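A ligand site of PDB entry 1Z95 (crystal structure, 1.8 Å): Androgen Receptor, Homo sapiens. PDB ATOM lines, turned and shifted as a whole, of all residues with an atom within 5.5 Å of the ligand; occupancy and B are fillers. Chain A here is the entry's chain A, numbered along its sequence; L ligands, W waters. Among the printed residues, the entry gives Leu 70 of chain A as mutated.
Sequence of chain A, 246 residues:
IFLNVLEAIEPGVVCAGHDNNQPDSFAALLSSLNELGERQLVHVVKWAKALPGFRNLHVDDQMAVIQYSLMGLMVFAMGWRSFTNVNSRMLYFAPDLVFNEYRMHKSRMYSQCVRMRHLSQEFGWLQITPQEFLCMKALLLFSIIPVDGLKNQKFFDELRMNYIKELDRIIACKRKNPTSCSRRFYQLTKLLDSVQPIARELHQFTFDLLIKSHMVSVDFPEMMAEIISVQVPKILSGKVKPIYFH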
ATOM      1  N   LEU A  30      30.351 -30.696  -4.715  1.00  0.00           N
ATOM      2  CA  LEU A  30      30.525 -29.932  -5.930  1.00  0.00           C
ATOM      3  C   LEU A  30      30.614 -30.779  -7.189  1.00  0.00           C
ATOM      4  O   LEU A  30      30.329 -30.289  -8.277  1.00  0.00           O
ATOM      5  CB  LEU A  30      31.698 -28.966  -5.789  1.00  0.00           C
ATOM      6  CG  LEU A  30      31.031 -27.703  -5.220  1.00  0.00           C
ATOM      7  CD1 LEU A  30      31.287 -27.604  -3.729  1.00  0.00           C
ATOM      8  CD2 LEU A  30      31.507 -26.499  -5.970  1.00  0.00           C
ATOM      9  N   LEU A  33      27.083 -30.994  -7.911  1.00  0.00           N
ATOM     10  CA  LEU A  33      26.540 -29.727  -8.415  1.00  0.00           C
ATOM     11  C   LEU A  33      26.963 -29.531  -9.861  1.00  0.00           C
ATOM     12  O   LEU A  33      26.206 -29.004 -10.677  1.00  0.00           O
ATOM     13  CB  LEU A  33      27.023 -28.537  -7.561  1.00  0.00           C
ATOM     14  CG  LEU A  33      26.226 -28.216  -6.290  1.00  0.00           C
ATOM     15  CD1 LEU A  33      26.866 -27.051  -5.539  1.00  0.00           C
ATOM     16  CD2 LEU A  33      24.787 -27.884  -6.665  1.00  0.00           C
ATOM     17  N   ASN A  34      28.191 -29.953 -10.183  1.00  0.00           N
ATOM     18  CA  ASN A  34      28.714 -29.836 -11.539  1.00  0.00           C
ATOM     19  C   ASN A  34      27.898 -30.737 -12.474  1.00  0.00           C
ATOM     20  O   ASN A  34      27.514 -30.320 -13.570  1.00  0.00           O
ATOM     21  CB  ASN A  34      30.195 -30.257 -11.573  1.00  0.00           C
ATOM     22  CG  ASN A  34      31.092 -29.277 -10.839  1.00  0.00           C
ATOM     23  OD1 ASN A  34      30.670 -28.171 -10.480  1.00  0.00           O
ATOM     24  ND2 ASN A  34      32.350 -29.659 -10.631  1.00  0.00           N
ATOM     25  N   GLU A  35      27.646 -31.961 -12.038  1.00  0.00           N
ATOM     26  CA  GLU A  35      26.861 -32.909 -12.839  1.00  0.00           C
ATOM     27  C   GLU A  35      25.453 -32.366 -13.060  1.00  0.00           C
ATOM     28  O   GLU A  35      24.912 -32.446 -14.154  1.00  0.00           O
ATOM     29  CB  GLU A  35      26.776 -34.275 -12.154  1.00  0.00           C
ATOM     30  CG  GLU A  35      25.864 -35.285 -12.860  1.00  0.00           C
ATOM     31  CD  GLU A  35      26.317 -35.618 -14.269  1.00  0.00           C
ATOM     32  OE1 GLU A  35      25.476 -36.096 -15.071  1.00  0.00           O
ATOM     33  OE2 GLU A  35      27.506 -35.413 -14.590  1.00  0.00           O
ATOM     34  N   LEU A  36      24.862 -31.798 -12.007  1.00  0.00           N
ATOM     35  CA  LEU A  36      23.518 -31.226 -12.106  1.00  0.00           C
ATOM     36  C   LEU A  36      23.503 -30.086 -13.117  1.00  0.00           C
ATOM     37  O   LEU A  36      22.539 -29.921 -13.869  1.00  0.00           O
ATOM     38  CB  LEU A  36      23.053 -30.701 -10.742  1.00  0.00           C
ATOM     39  CG  LEU A  36      21.609 -30.170 -10.722  1.00  0.00           C
ATOM     40  CD1 LEU A  36      20.670 -31.270 -11.189  1.00  0.00           C
ATOM     41  CD2 LEU A  36      21.240 -29.710  -9.319  1.00  0.00           C
ATOM     42  N   GLY A  37      24.572 -29.291 -13.126  1.00  0.00           N
ATOM     43  CA  GLY A  37      24.640 -28.187 -14.067  1.00  0.00           C
ATOM     44  C   GLY A  37      24.622 -28.766 -15.475  1.00  0.00           C
ATOM     45  O   GLY A  37      23.917 -28.274 -16.349  1.00  0.00           O
ATOM     46  N   GLU A  38      25.381 -29.840 -15.670  1.00  0.00           N
ATOM     47  CA  GLU A  38      25.444 -30.499 -16.964  1.00  0.00           C
ATOM     48  C   GLU A  38      24.040 -30.982 -17.363  1.00  0.00           C
ATOM     49  O   GLU A  38      23.622 -30.828 -18.515  1.00  0.00           O
ATOM     50  CB  GLU A  38      26.404 -31.701 -16.891  1.00  0.00           C
ATOM     51  CG  GLU A  38      26.675 -32.377 -18.237  1.00  0.00           C
ATOM     52  CD  GLU A  38      27.781 -31.684 -19.018  1.00  0.00           C
ATOM     53  OE1 GLU A  38      28.129 -30.535 -18.667  1.00  0.00           O
ATOM     54  OE2 GLU A  38      28.292 -32.286 -19.984  1.00  0.00           O
ATOM     55  N   GLN A  40      21.020 -29.838 -16.151  1.00  0.00           N
ATOM     56  CA  GLN A  40      20.078 -28.747 -16.340  1.00  0.00           C
ATOM     57  C   GLN A  40      20.343 -28.021 -17.652  1.00  0.00           C
ATOM     58  O   GLN A  40      19.410 -27.525 -18.281  1.00  0.00           O
ATOM     59  CB  GLN A  40      20.108 -27.770 -15.158  1.00  0.00           C
ATOM     60  CG  GLN A  40      19.668 -28.423 -13.843  1.00  0.00           C
ATOM     61  CD  GLN A  40      19.297 -27.447 -12.754  1.00  0.00           C
ATOM     62  OE1 GLN A  40      18.949 -27.853 -11.642  1.00  0.00           O
ATOM     63  NE2 GLN A  40      19.354 -26.154 -13.048  1.00  0.00           N
ATOM     64  N   GLN A  67      24.525 -20.019 -22.957  1.00  0.00           N
ATOM     65  CA  GLN A  67      25.690 -20.276 -22.103  1.00  0.00           C
ATOM     66  C   GLN A  67      25.988 -19.115 -21.144  1.00  0.00           C
ATOM     67  O   GLN A  67      26.338 -19.341 -19.987  1.00  0.00           O
ATOM     68  CB  GLN A  67      26.904 -20.571 -22.970  1.00  0.00           C
ATOM     69  CG  GLN A  67      26.722 -21.785 -23.860  1.00  0.00           C
ATOM     70  CD  GLN A  67      27.922 -22.078 -24.725  1.00  0.00           C
ATOM     71  OE1 GLN A  67      28.491 -21.171 -25.345  1.00  0.00           O
ATOM     72  NE2 GLN A  67      28.306 -23.339 -24.802  1.00  0.00           N
ATOM     73  N   LEU A  70      23.095 -19.161 -18.484  1.00  0.00           N
ATOM     74  CA  LEU A  70      22.815 -20.414 -17.770  1.00  0.00           C
ATOM     75  C   LEU A  70      22.838 -20.261 -16.251  1.00  0.00           C
ATOM     76  O   LEU A  70      21.893 -20.674 -15.573  1.00  0.00           O
ATOM     77  CB  LEU A  70      23.802 -21.509 -18.185  1.00  0.00           C
ATOM     78  CG  LEU A  70      23.666 -22.865 -17.469  1.00  0.00           C
ATOM     79  CD1 LEU A  70      22.329 -23.501 -17.836  1.00  0.00           C
ATOM     80  CD2 LEU A  70      24.812 -23.789 -17.865  1.00  0.00           C
ATOM     81  N   MET A  71      23.903 -19.671 -15.704  1.00  0.00           N
ATOM     82  CA  MET A  71      23.986 -19.543 -14.249  1.00  0.00           C
ATOM     83  C   MET A  71      22.778 -18.827 -13.628  1.00  0.00           C
ATOM     84  O   MET A  71      22.158 -19.347 -12.696  1.00  0.00           O
ATOM     85  CB  MET A  71      25.276 -18.837 -13.826  1.00  0.00           C
ATOM     86  CG  MET A  71      25.554 -18.933 -12.316  1.00  0.00           C
ATOM     87  SD  MET A  71      25.885 -20.627 -11.765  1.00  0.00           S
ATOM     88  CE  MET A  71      27.697 -20.711 -12.047  1.00  0.00           C
ATOM     89  N   MET A  74      19.504 -20.807 -13.889  1.00  0.00           N
ATOM     90  CA  MET A  74      19.478 -21.898 -12.916  1.00  0.00           C
ATOM     91  C   MET A  74      19.233 -21.390 -11.499  1.00  0.00           C
ATOM     92  O   MET A  74      18.532 -22.032 -10.722  1.00  0.00           O
ATOM     93  CB  MET A  74      20.783 -22.691 -12.965  1.00  0.00           C
ATOM     94  CG  MET A  74      21.046 -23.439 -14.274  1.00  0.00           C
ATOM     95  SD  MET A  74      22.330 -24.689 -14.040  1.00  0.00           S
ATOM     96  CE  MET A  74      23.736 -23.660 -13.843  1.00  0.00           C
ATOM     97  N   VAL A  75      19.806 -20.227 -11.159  1.00  0.00           N
ATOM     98  CA  VAL A  75      19.644 -19.622  -9.836  1.00  0.00           C
ATOM     99  C   VAL A  75      18.193 -19.215  -9.611  1.00  0.00           C
ATOM    100  O   VAL A  75      17.612 -19.498  -8.556  1.00  0.00           O
ATOM    101  CB  VAL A  75      20.541 -18.351  -9.686  1.00  0.00           C
ATOM    102  CG1 VAL A  75      20.066 -17.527  -8.489  1.00  0.00           C
ATOM    103  CG2 VAL A  75      21.996 -18.757  -9.487  1.00  0.00           C
ATOM    104  N   MET A  78      15.953 -22.195  -9.357  1.00  0.00           N
ATOM    105  CA  MET A  78      16.239 -22.866  -8.099  1.00  0.00           C
ATOM    106  C   MET A  78      15.564 -22.142  -6.923  1.00  0.00           C
ATOM    107  O   MET A  78      15.015 -22.780  -6.031  1.00  0.00           O
ATOM    108  CB  MET A  78      17.746 -22.961  -7.873  1.00  0.00           C
ATOM    109  CG  MET A  78      18.165 -23.882  -6.727  1.00  0.00           C
ATOM    110  SD  MET A  78      18.121 -23.086  -5.112  1.00  0.00           S
ATOM    111  CE  MET A  78      19.538 -21.968  -5.285  1.00  0.00           C
ATOM    112  N   ARG A  81      11.917 -23.016  -6.898  1.00  0.00           N
ATOM    113  CA  ARG A  81      11.653 -24.378  -6.440  1.00  0.00           C
ATOM    114  C   ARG A  81      11.767 -24.461  -4.929  1.00  0.00           C
ATOM    115  O   ARG A  81      10.938 -25.086  -4.268  1.00  0.00           O
ATOM    116  CB  ARG A  81      12.633 -25.377  -7.078  1.00  0.00           C
ATOM    117  CG  ARG A  81      12.386 -25.669  -8.547  1.00  0.00           C
ATOM    118  CD  ARG A  81      13.136 -26.928  -8.975  1.00  0.00           C
ATOM    119  NE  ARG A  81      14.582 -26.805  -8.765  1.00  0.00           N
ATOM    120  CZ  ARG A  81      15.396 -26.123  -9.555  1.00  0.00           C
ATOM    121  NH1 ARG A  81      14.924 -25.505 -10.629  1.00  0.00           N
ATOM    122  NH2 ARG A  81      16.689 -26.066  -9.275  1.00  0.00           N
ATOM    123  N   TYR A  92      16.799 -25.968  -2.530  1.00  0.00           N
ATOM    124  CA  TYR A  92      16.353 -27.118  -3.313  1.00  0.00           C
ATOM    125  C   TYR A  92      16.992 -27.196  -4.711  1.00  0.00           C
ATOM    126  O   TYR A  92      16.318 -26.958  -5.709  1.00  0.00           O
ATOM    127  CB  TYR A  92      14.826 -27.047  -3.435  1.00  0.00           C
ATOM    128  CG  TYR A  92      14.122 -28.357  -3.663  1.00  0.00           C
ATOM    129  CD1 TYR A  92      13.857 -29.218  -2.588  1.00  0.00           C
ATOM    130  CD2 TYR A  92      13.697 -28.744  -4.938  1.00  0.00           C
ATOM    131  CE1 TYR A  92      13.180 -30.425  -2.787  1.00  0.00           C
ATOM    132  CE2 TYR A  92      13.020 -29.946  -5.146  1.00  0.00           C
ATOM    133  CZ  TYR A  92      12.765 -30.784  -4.070  1.00  0.00           C
ATOM    134  OH  TYR A  92      12.093 -31.962  -4.263  1.00  0.00           O
ATOM    135  N   PHE A  93      18.277 -27.544  -4.789  1.00  0.00           N
ATOM    136  CA  PHE A  93      18.932 -27.648  -6.085  1.00  0.00           C
ATOM    137  C   PHE A  93      18.272 -28.718  -6.942  1.00  0.00           C
ATOM    138  O   PHE A  93      18.055 -28.527  -8.148  1.00  0.00           O
ATOM    139  CB  PHE A  93      20.416 -27.984  -5.914  1.00  0.00           C
ATOM    140  CG  PHE A  93      21.203 -26.868  -5.304  1.00  0.00           C
ATOM    141  CD1 PHE A  93      21.466 -26.855  -3.937  1.00  0.00           C
ATOM    142  CD2 PHE A  93      21.658 -25.816  -6.089  1.00  0.00           C
ATOM    143  CE1 PHE A  93      22.175 -25.795  -3.359  1.00  0.00           C
ATOM    144  CE2 PHE A  93      22.359 -24.755  -5.522  1.00  0.00           C
ATOM    145  CZ  PHE A  93      22.622 -24.748  -4.147  1.00  0.00           C
ATOM    146  N   MET A 109      30.335 -22.511  -0.162  1.00  0.00           N
ATOM    147  CA  MET A 109      29.541 -21.536  -0.922  1.00  0.00           C
ATOM    148  C   MET A 109      28.497 -20.956   0.023  1.00  0.00           C
ATOM    149  O   MET A 109      27.420 -20.535  -0.402  1.00  0.00           O
ATOM    150  CB  MET A 109      28.801 -22.246  -2.059  1.00  0.00           C
ATOM    151  CG  MET A 109      29.644 -23.137  -2.944  1.00  0.00           C
ATOM    152  SD  MET A 109      28.594 -24.077  -4.085  1.00  0.00           S
ATOM    153  CE  MET A 109      28.008 -22.748  -5.114  1.00  0.00           C
ATOM    154  N   MET A 116      21.182 -16.623  -2.202  1.00  0.00           N
ATOM    155  CA  MET A 116      20.209 -17.366  -2.976  1.00  0.00           C
ATOM    156  C   MET A 116      18.943 -17.629  -2.172  1.00  0.00           C
ATOM    157  O   MET A 116      17.846 -17.636  -2.732  1.00  0.00           O
ATOM    158  CB  MET A 116      20.795 -18.689  -3.486  1.00  0.00           C
ATOM    159  CG  MET A 116      21.769 -18.489  -4.639  1.00  0.00           C
ATOM    160  SD  MET A 116      22.355 -20.029  -5.389  1.00  0.00           S
ATOM    161  CE  MET A 116      23.771 -20.376  -4.375  1.00  0.00           C
ATOM    162  N   LEU A 202      28.858 -16.779  -8.298  1.00  0.00           N
ATOM    163  CA  LEU A 202      28.911 -18.197  -8.627  1.00  0.00           C
ATOM    164  C   LEU A 202      29.873 -18.424  -9.797  1.00  0.00           C
ATOM    165  O   LEU A 202      30.592 -19.422  -9.826  1.00  0.00           O
ATOM    166  CB  LEU A 202      27.508 -18.706  -8.983  1.00  0.00           C
ATOM    167  CG  LEU A 202      26.547 -18.753  -7.806  1.00  0.00           C
ATOM    168  CD1 LEU A 202      25.148 -19.101  -8.275  1.00  0.00           C
ATOM    169  CD2 LEU A 202      27.034 -19.771  -6.804  1.00  0.00           C
ATOM    170  N   HIS A 203      29.857 -17.515 -10.763  1.00  0.00           N
ATOM    171  CA  HIS A 203      30.734 -17.600 -11.925  1.00  0.00           C
ATOM    172  C   HIS A 203      32.194 -17.538 -11.470  1.00  0.00           C
ATOM    173  O   HIS A 203      33.029 -18.326 -11.926  1.00  0.00           O
ATOM    174  CB  HIS A 203      30.452 -16.433 -12.864  1.00  0.00           C
ATOM    175  CG  HIS A 203      29.354 -16.693 -13.852  1.00  0.00           C
ATOM    176  ND1 HIS A 203      28.549 -15.690 -14.336  1.00  0.00           N
ATOM    177  CD2 HIS A 203      28.986 -17.826 -14.498  1.00  0.00           C
ATOM    178  CE1 HIS A 203      27.725 -16.196 -15.249  1.00  0.00           C
ATOM    179  NE2 HIS A 203      27.977 -17.482 -15.361  1.00  0.00           N
ATOM    180  N   PHE A 205      33.409 -18.158  -8.418  1.00  0.00           N
ATOM    181  CA  PHE A 205      33.678 -19.345  -7.621  1.00  0.00           C
ATOM    182  C   PHE A 205      33.898 -20.571  -8.507  1.00  0.00           C
ATOM    183  O   PHE A 205      34.834 -21.350  -8.300  1.00  0.00           O
ATOM    184  CB  PHE A 205      32.525 -19.572  -6.644  1.00  0.00           C
ATOM    185  CG  PHE A 205      32.546 -20.912  -5.958  1.00  0.00           C
ATOM    186  CD1 PHE A 205      32.009 -22.036  -6.581  1.00  0.00           C
ATOM    187  CD2 PHE A 205      33.103 -21.055  -4.698  1.00  0.00           C
ATOM    188  CE1 PHE A 205      32.024 -23.274  -5.949  1.00  0.00           C
ATOM    189  CE2 PHE A 205      33.127 -22.294  -4.054  1.00  0.00           C
ATOM    190  CZ  PHE A 205      32.584 -23.406  -4.682  1.00  0.00           C
ATOM    191  N   THR A 206      33.038 -20.733  -9.512  1.00  0.00           N
ATOM    192  CA  THR A 206      33.118 -21.854 -10.446  1.00  0.00           C
ATOM    193  C   THR A 206      34.418 -21.836 -11.250  1.00  0.00           C
ATOM    194  O   THR A 206      35.042 -22.869 -11.475  1.00  0.00           O
ATOM    195  CB  THR A 206      31.931 -21.819 -11.425  1.00  0.00           C
ATOM    196  OG1 THR A 206      30.705 -21.948 -10.691  1.00  0.00           O
ATOM    197  CG2 THR A 206      32.042 -22.951 -12.437  1.00  0.00           C
ATOM    198  N   LEU A 209      37.310 -22.713  -9.043  1.00  0.00           N
ATOM    199  CA  LEU A 209      37.235 -24.130  -8.732  1.00  0.00           C
ATOM    200  C   LEU A 209      37.745 -25.002  -9.878  1.00  0.00           C
ATOM    201  O   LEU A 209      38.451 -25.980  -9.646  1.00  0.00           O
ATOM    202  CB  LEU A 209      35.802 -24.531  -8.384  1.00  0.00           C
ATOM    203  CG  LEU A 209      35.692 -25.983  -7.906  1.00  0.00           C
ATOM    204  CD1 LEU A 209      36.557 -26.173  -6.660  1.00  0.00           C
ATOM    205  CD2 LEU A 209      34.240 -26.316  -7.621  1.00  0.00           C
ATOM    206  N   PHE A 220      34.531 -32.151 -13.197  1.00  0.00           N
ATOM    207  CA  PHE A 220      33.700 -31.294 -14.041  1.00  0.00           C
ATOM    208  C   PHE A 220      33.356 -32.015 -15.338  1.00  0.00           C
ATOM    209  O   PHE A 220      34.243 -32.507 -16.035  1.00  0.00           O
ATOM    210  CB  PHE A 220      34.433 -30.001 -14.414  1.00  0.00           C
ATOM    211  CG  PHE A 220      34.423 -28.957 -13.341  1.00  0.00           C
ATOM    212  CD1 PHE A 220      35.407 -28.950 -12.365  1.00  0.00           C
ATOM    213  CD2 PHE A 220      33.441 -27.979 -13.317  1.00  0.00           C
ATOM    214  CE1 PHE A 220      35.409 -27.970 -11.357  1.00  0.00           C
ATOM    215  CE2 PHE A 220      33.433 -26.993 -12.328  1.00  0.00           C
ATOM    216  CZ  PHE A 220      34.417 -26.992 -11.343  1.00  0.00           C
ATOM    217  N   MET A 224      30.476 -28.518 -19.157  1.00  0.00           N
ATOM    218  CA  MET A 224      30.616 -27.494 -18.136  1.00  0.00           C
ATOM    219  C   MET A 224      32.040 -26.946 -18.168  1.00  0.00           C
ATOM    220  O   MET A 224      32.242 -25.744 -18.123  1.00  0.00           O
ATOM    221  CB  MET A 224      30.287 -28.083 -16.761  1.00  0.00           C
ATOM    222  CG  MET A 224      28.914 -28.725 -16.719  1.00  0.00           C
ATOM    223  SD  MET A 224      27.678 -27.736 -17.622  1.00  0.00           S
ATOM    224  CE  MET A 224      27.384 -26.515 -16.396  1.00  0.00           C
ATOM    225  N   ILE A 227      32.373 -24.543 -21.066  1.00  0.00           N
ATOM    226  CA  ILE A 227      31.710 -23.274 -20.812  1.00  0.00           C
ATOM    227  C   ILE A 227      32.446 -22.418 -19.772  1.00  0.00           C
ATOM    228  O   ILE A 227      32.553 -21.210 -19.920  1.00  0.00           O
ATOM    229  CB  ILE A 227      30.244 -23.479 -20.342  1.00  0.00           C
ATOM    230  CG1 ILE A 227      29.400 -24.074 -21.475  1.00  0.00           C
ATOM    231  CG2 ILE A 227      29.635 -22.152 -19.912  1.00  0.00           C
ATOM    232  CD1 ILE A 227      27.956 -24.358 -21.079  1.00  0.00           C
ATOM    233  N   ILE A 228      32.977 -23.059 -18.726  1.00  0.00           N
ATOM    234  CA  ILE A 228      33.681 -22.321 -17.676  1.00  0.00           C
ATOM    235  C   ILE A 228      34.994 -21.727 -18.182  1.00  0.00           C
ATOM    236  O   ILE A 228      35.392 -20.648 -17.748  1.00  0.00           O
ATOM    237  CB  ILE A 228      33.980 -23.237 -16.464  1.00  0.00           C
ATOM    238  CG1 ILE A 228      32.668 -23.729 -15.848  1.00  0.00           C
ATOM    239  CG2 ILE A 228      34.809 -22.487 -15.411  1.00  0.00           C
ATOM    240  CD1 ILE A 228      32.853 -24.912 -14.916  1.00  0.00           C
ATOM    241  N   VAL A 232      32.709 -18.222 -19.553  1.00  0.00           N
ATOM    242  CA  VAL A 232      32.773 -17.540 -18.248  1.00  0.00           C
ATOM    243  C   VAL A 232      33.909 -16.529 -18.113  1.00  0.00           C
ATOM    244  O   VAL A 232      33.729 -15.474 -17.488  1.00  0.00           O
ATOM    245  CB  VAL A 232      32.831 -18.571 -17.088  1.00  0.00           C
ATOM    246  CG1 VAL A 232      32.998 -17.866 -15.737  1.00  0.00           C
ATOM    247  CG2 VAL A 232      31.552 -19.422 -17.073  1.00  0.00           C
HETATM  248  C1  LIG L   1      27.130 -23.353 -14.142  1.00  0.00           C
HETATM  249  C2  LIG L   1      26.992 -22.284 -15.017  1.00  0.00           C
HETATM  250  C3  LIG L   1      27.972 -22.030 -15.960  1.00  0.00           C
HETATM  251  F1  LIG L   1      27.846 -20.991 -16.818  1.00  0.00           F
HETATM  252  C4  LIG L   1      29.096 -22.846 -16.041  1.00  0.00           C
HETATM  253  C5  LIG L   1      29.240 -23.922 -15.170  1.00  0.00           C
HETATM  254  C6  LIG L   1      28.259 -24.181 -14.219  1.00  0.00           C
HETATM  255  S1  LIG L   1      28.459 -25.512 -13.108  1.00  0.00           S
HETATM  256  O1  LIG L   1      27.111 -26.110 -12.816  1.00  0.00           O
HETATM  257  O2  LIG L   1      29.349 -26.549 -13.732  1.00  0.00           O
HETATM  258  C7  LIG L   1      29.220 -24.904 -11.564  1.00  0.00           C
HETATM  259  C8  LIG L   1      28.575 -25.417 -10.274  1.00  0.00           C
HETATM  260  O3  LIG L   1      28.509 -26.851 -10.326  1.00  0.00           O
HETATM  261  C9  LIG L   1      29.390 -24.982  -9.063  1.00  0.00           C
HETATM  262  C10 LIG L   1      27.148 -24.874 -10.142  1.00  0.00           C
HETATM  263  O4  LIG L   1      26.949 -23.655 -10.039  1.00  0.00           O
HETATM  264  N1  LIG L   1      26.194 -25.790 -10.270  1.00  0.00           N
HETATM  265  C11 LIG L   1      24.890 -25.589 -10.165  1.00  0.00           C
HETATM  266  C12 LIG L   1      24.331 -24.382  -9.753  1.00  0.00           C
HETATM  267  C13 LIG L   1      24.050 -26.679 -10.370  1.00  0.00           C
HETATM  268  C14 LIG L   1      22.677 -26.537 -10.170  1.00  0.00           C
HETATM  269  C15 LIG L   1      22.140 -25.323  -9.765  1.00  0.00           C
HETATM  270  C16 LIG L   1      20.709 -25.281  -9.614  1.00  0.00           C
HETATM  271  N2  LIG L   1      19.579 -25.264  -9.499  1.00  0.00           N
HETATM  272  C17 LIG L   1      22.963 -24.217  -9.539  1.00  0.00           C
HETATM  273  C18 LIG L   1      22.441 -22.846  -9.048  1.00  0.00           C
HETATM  274  F2  LIG L   1      22.169 -22.074 -10.092  1.00  0.00           F
HETATM  275  F3  LIG L   1      21.342 -22.910  -8.302  1.00  0.00           F
HETATM  276  F4  LIG L   1      23.337 -22.210  -8.292  1.00  0.00           F
HETATM  277  O   HOH W   1      17.648 -24.450 -11.668  1.00  0.00           O
HETATM  278  O   HOH W   2      26.175 -18.640 -17.263  1.00  0.00           O
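The side-chain amide oxygen of Asn 34 sits close to the backbone carbonyl oxygen of Leu 30 (3.1 Å).
O of Phe 93 lies within hydrogen-bond range of NH2 of Arg 81 (3.0 Å).
The side-chain sulfur of Met 74 sits close to the side-chain amide nitrogen of Gln 40 (3.5 Å).
The backbone NH (N) of Met 224 sits close to the side-chain carboxylate (OE1) of Glu 38, at 3.1 Å.
The backbone carbonyl oxygen (O) of Leu 202 lies within hydrogen-bond range of the side-chain hydroxyl (OG1) of Thr 206, 2.7 Å away.
The backbone carbonyl oxygen (O) of Ile 227 sits at hydrogen-bond distance from the backbone NH (N) of Val 232, 3.0 Å away.
N of Asn 34 sits at hydrogen-bond distance from O3 of the ligand (3.1 Å).
The side-chain amide oxygen (OD1) of Asn 34 lies within hydrogen-bond range of an oxygen (O3) of the ligand (2.5 Å).
The guanidinium group of Arg 81 lies within hydrogen-bond range of a nitrogen (N2) of the ligand (3.0 Å).
O3 of the ligand lies close to O of Leu 33, 3.2 Å away.
A nitrogen (N2) of the ligand sits close to the side-chain amide oxygen of Gln 40, 3.4 Å away.
Water W2 lies within hydrogen-bond range of the backbone carbonyl oxygen of Gln 67, a ring nitrogen (NE2) of His 203, the backbone NH of Met 71 and the backbone NH of Leu 70.
Water W1 lies within hydrogen-bond range of the backbone carbonyl oxygen of Met 74 (2.7 Å), the side-chain amide nitrogen of Gln 40 (2.8 Å), a nitrogen (N2) of the ligand (3.0 Å) and the guanidinium group of Arg 81 (3.0 Å).
O4 of the ligand lies close to SD of Met 71.
F2 of the ligand lies close to N of Val 75 (3.2 Å).
SD of Met 116 lies close to F4 of the ligand.
Merely in contact with the ligand: Leu 36 (3.6 Å), Gly 37 (3.5 Å), Gln 67 (3.9 Å), Leu 70 (3.9 Å), Met 74 (3.2 Å), Met 78 (3.4 Å), Phe 93 (3.5 Å), Leu 202 (3.6 Å), His 203 (3.8 Å), Thr 206 (3.4 Å), Met 224 (3.3 Å), Ile 227 (3.8 Å) and Ile 228 (3.5 Å).
Hydrophobic or aromatic side chains within 4 Å of the ligand: Leu 33, Leu 36, Leu 70, Met 71, Met 74, Val 75, Met 78, Phe 93, Met 116, Leu 202, Met 224, Ile 227 and Ile 228.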
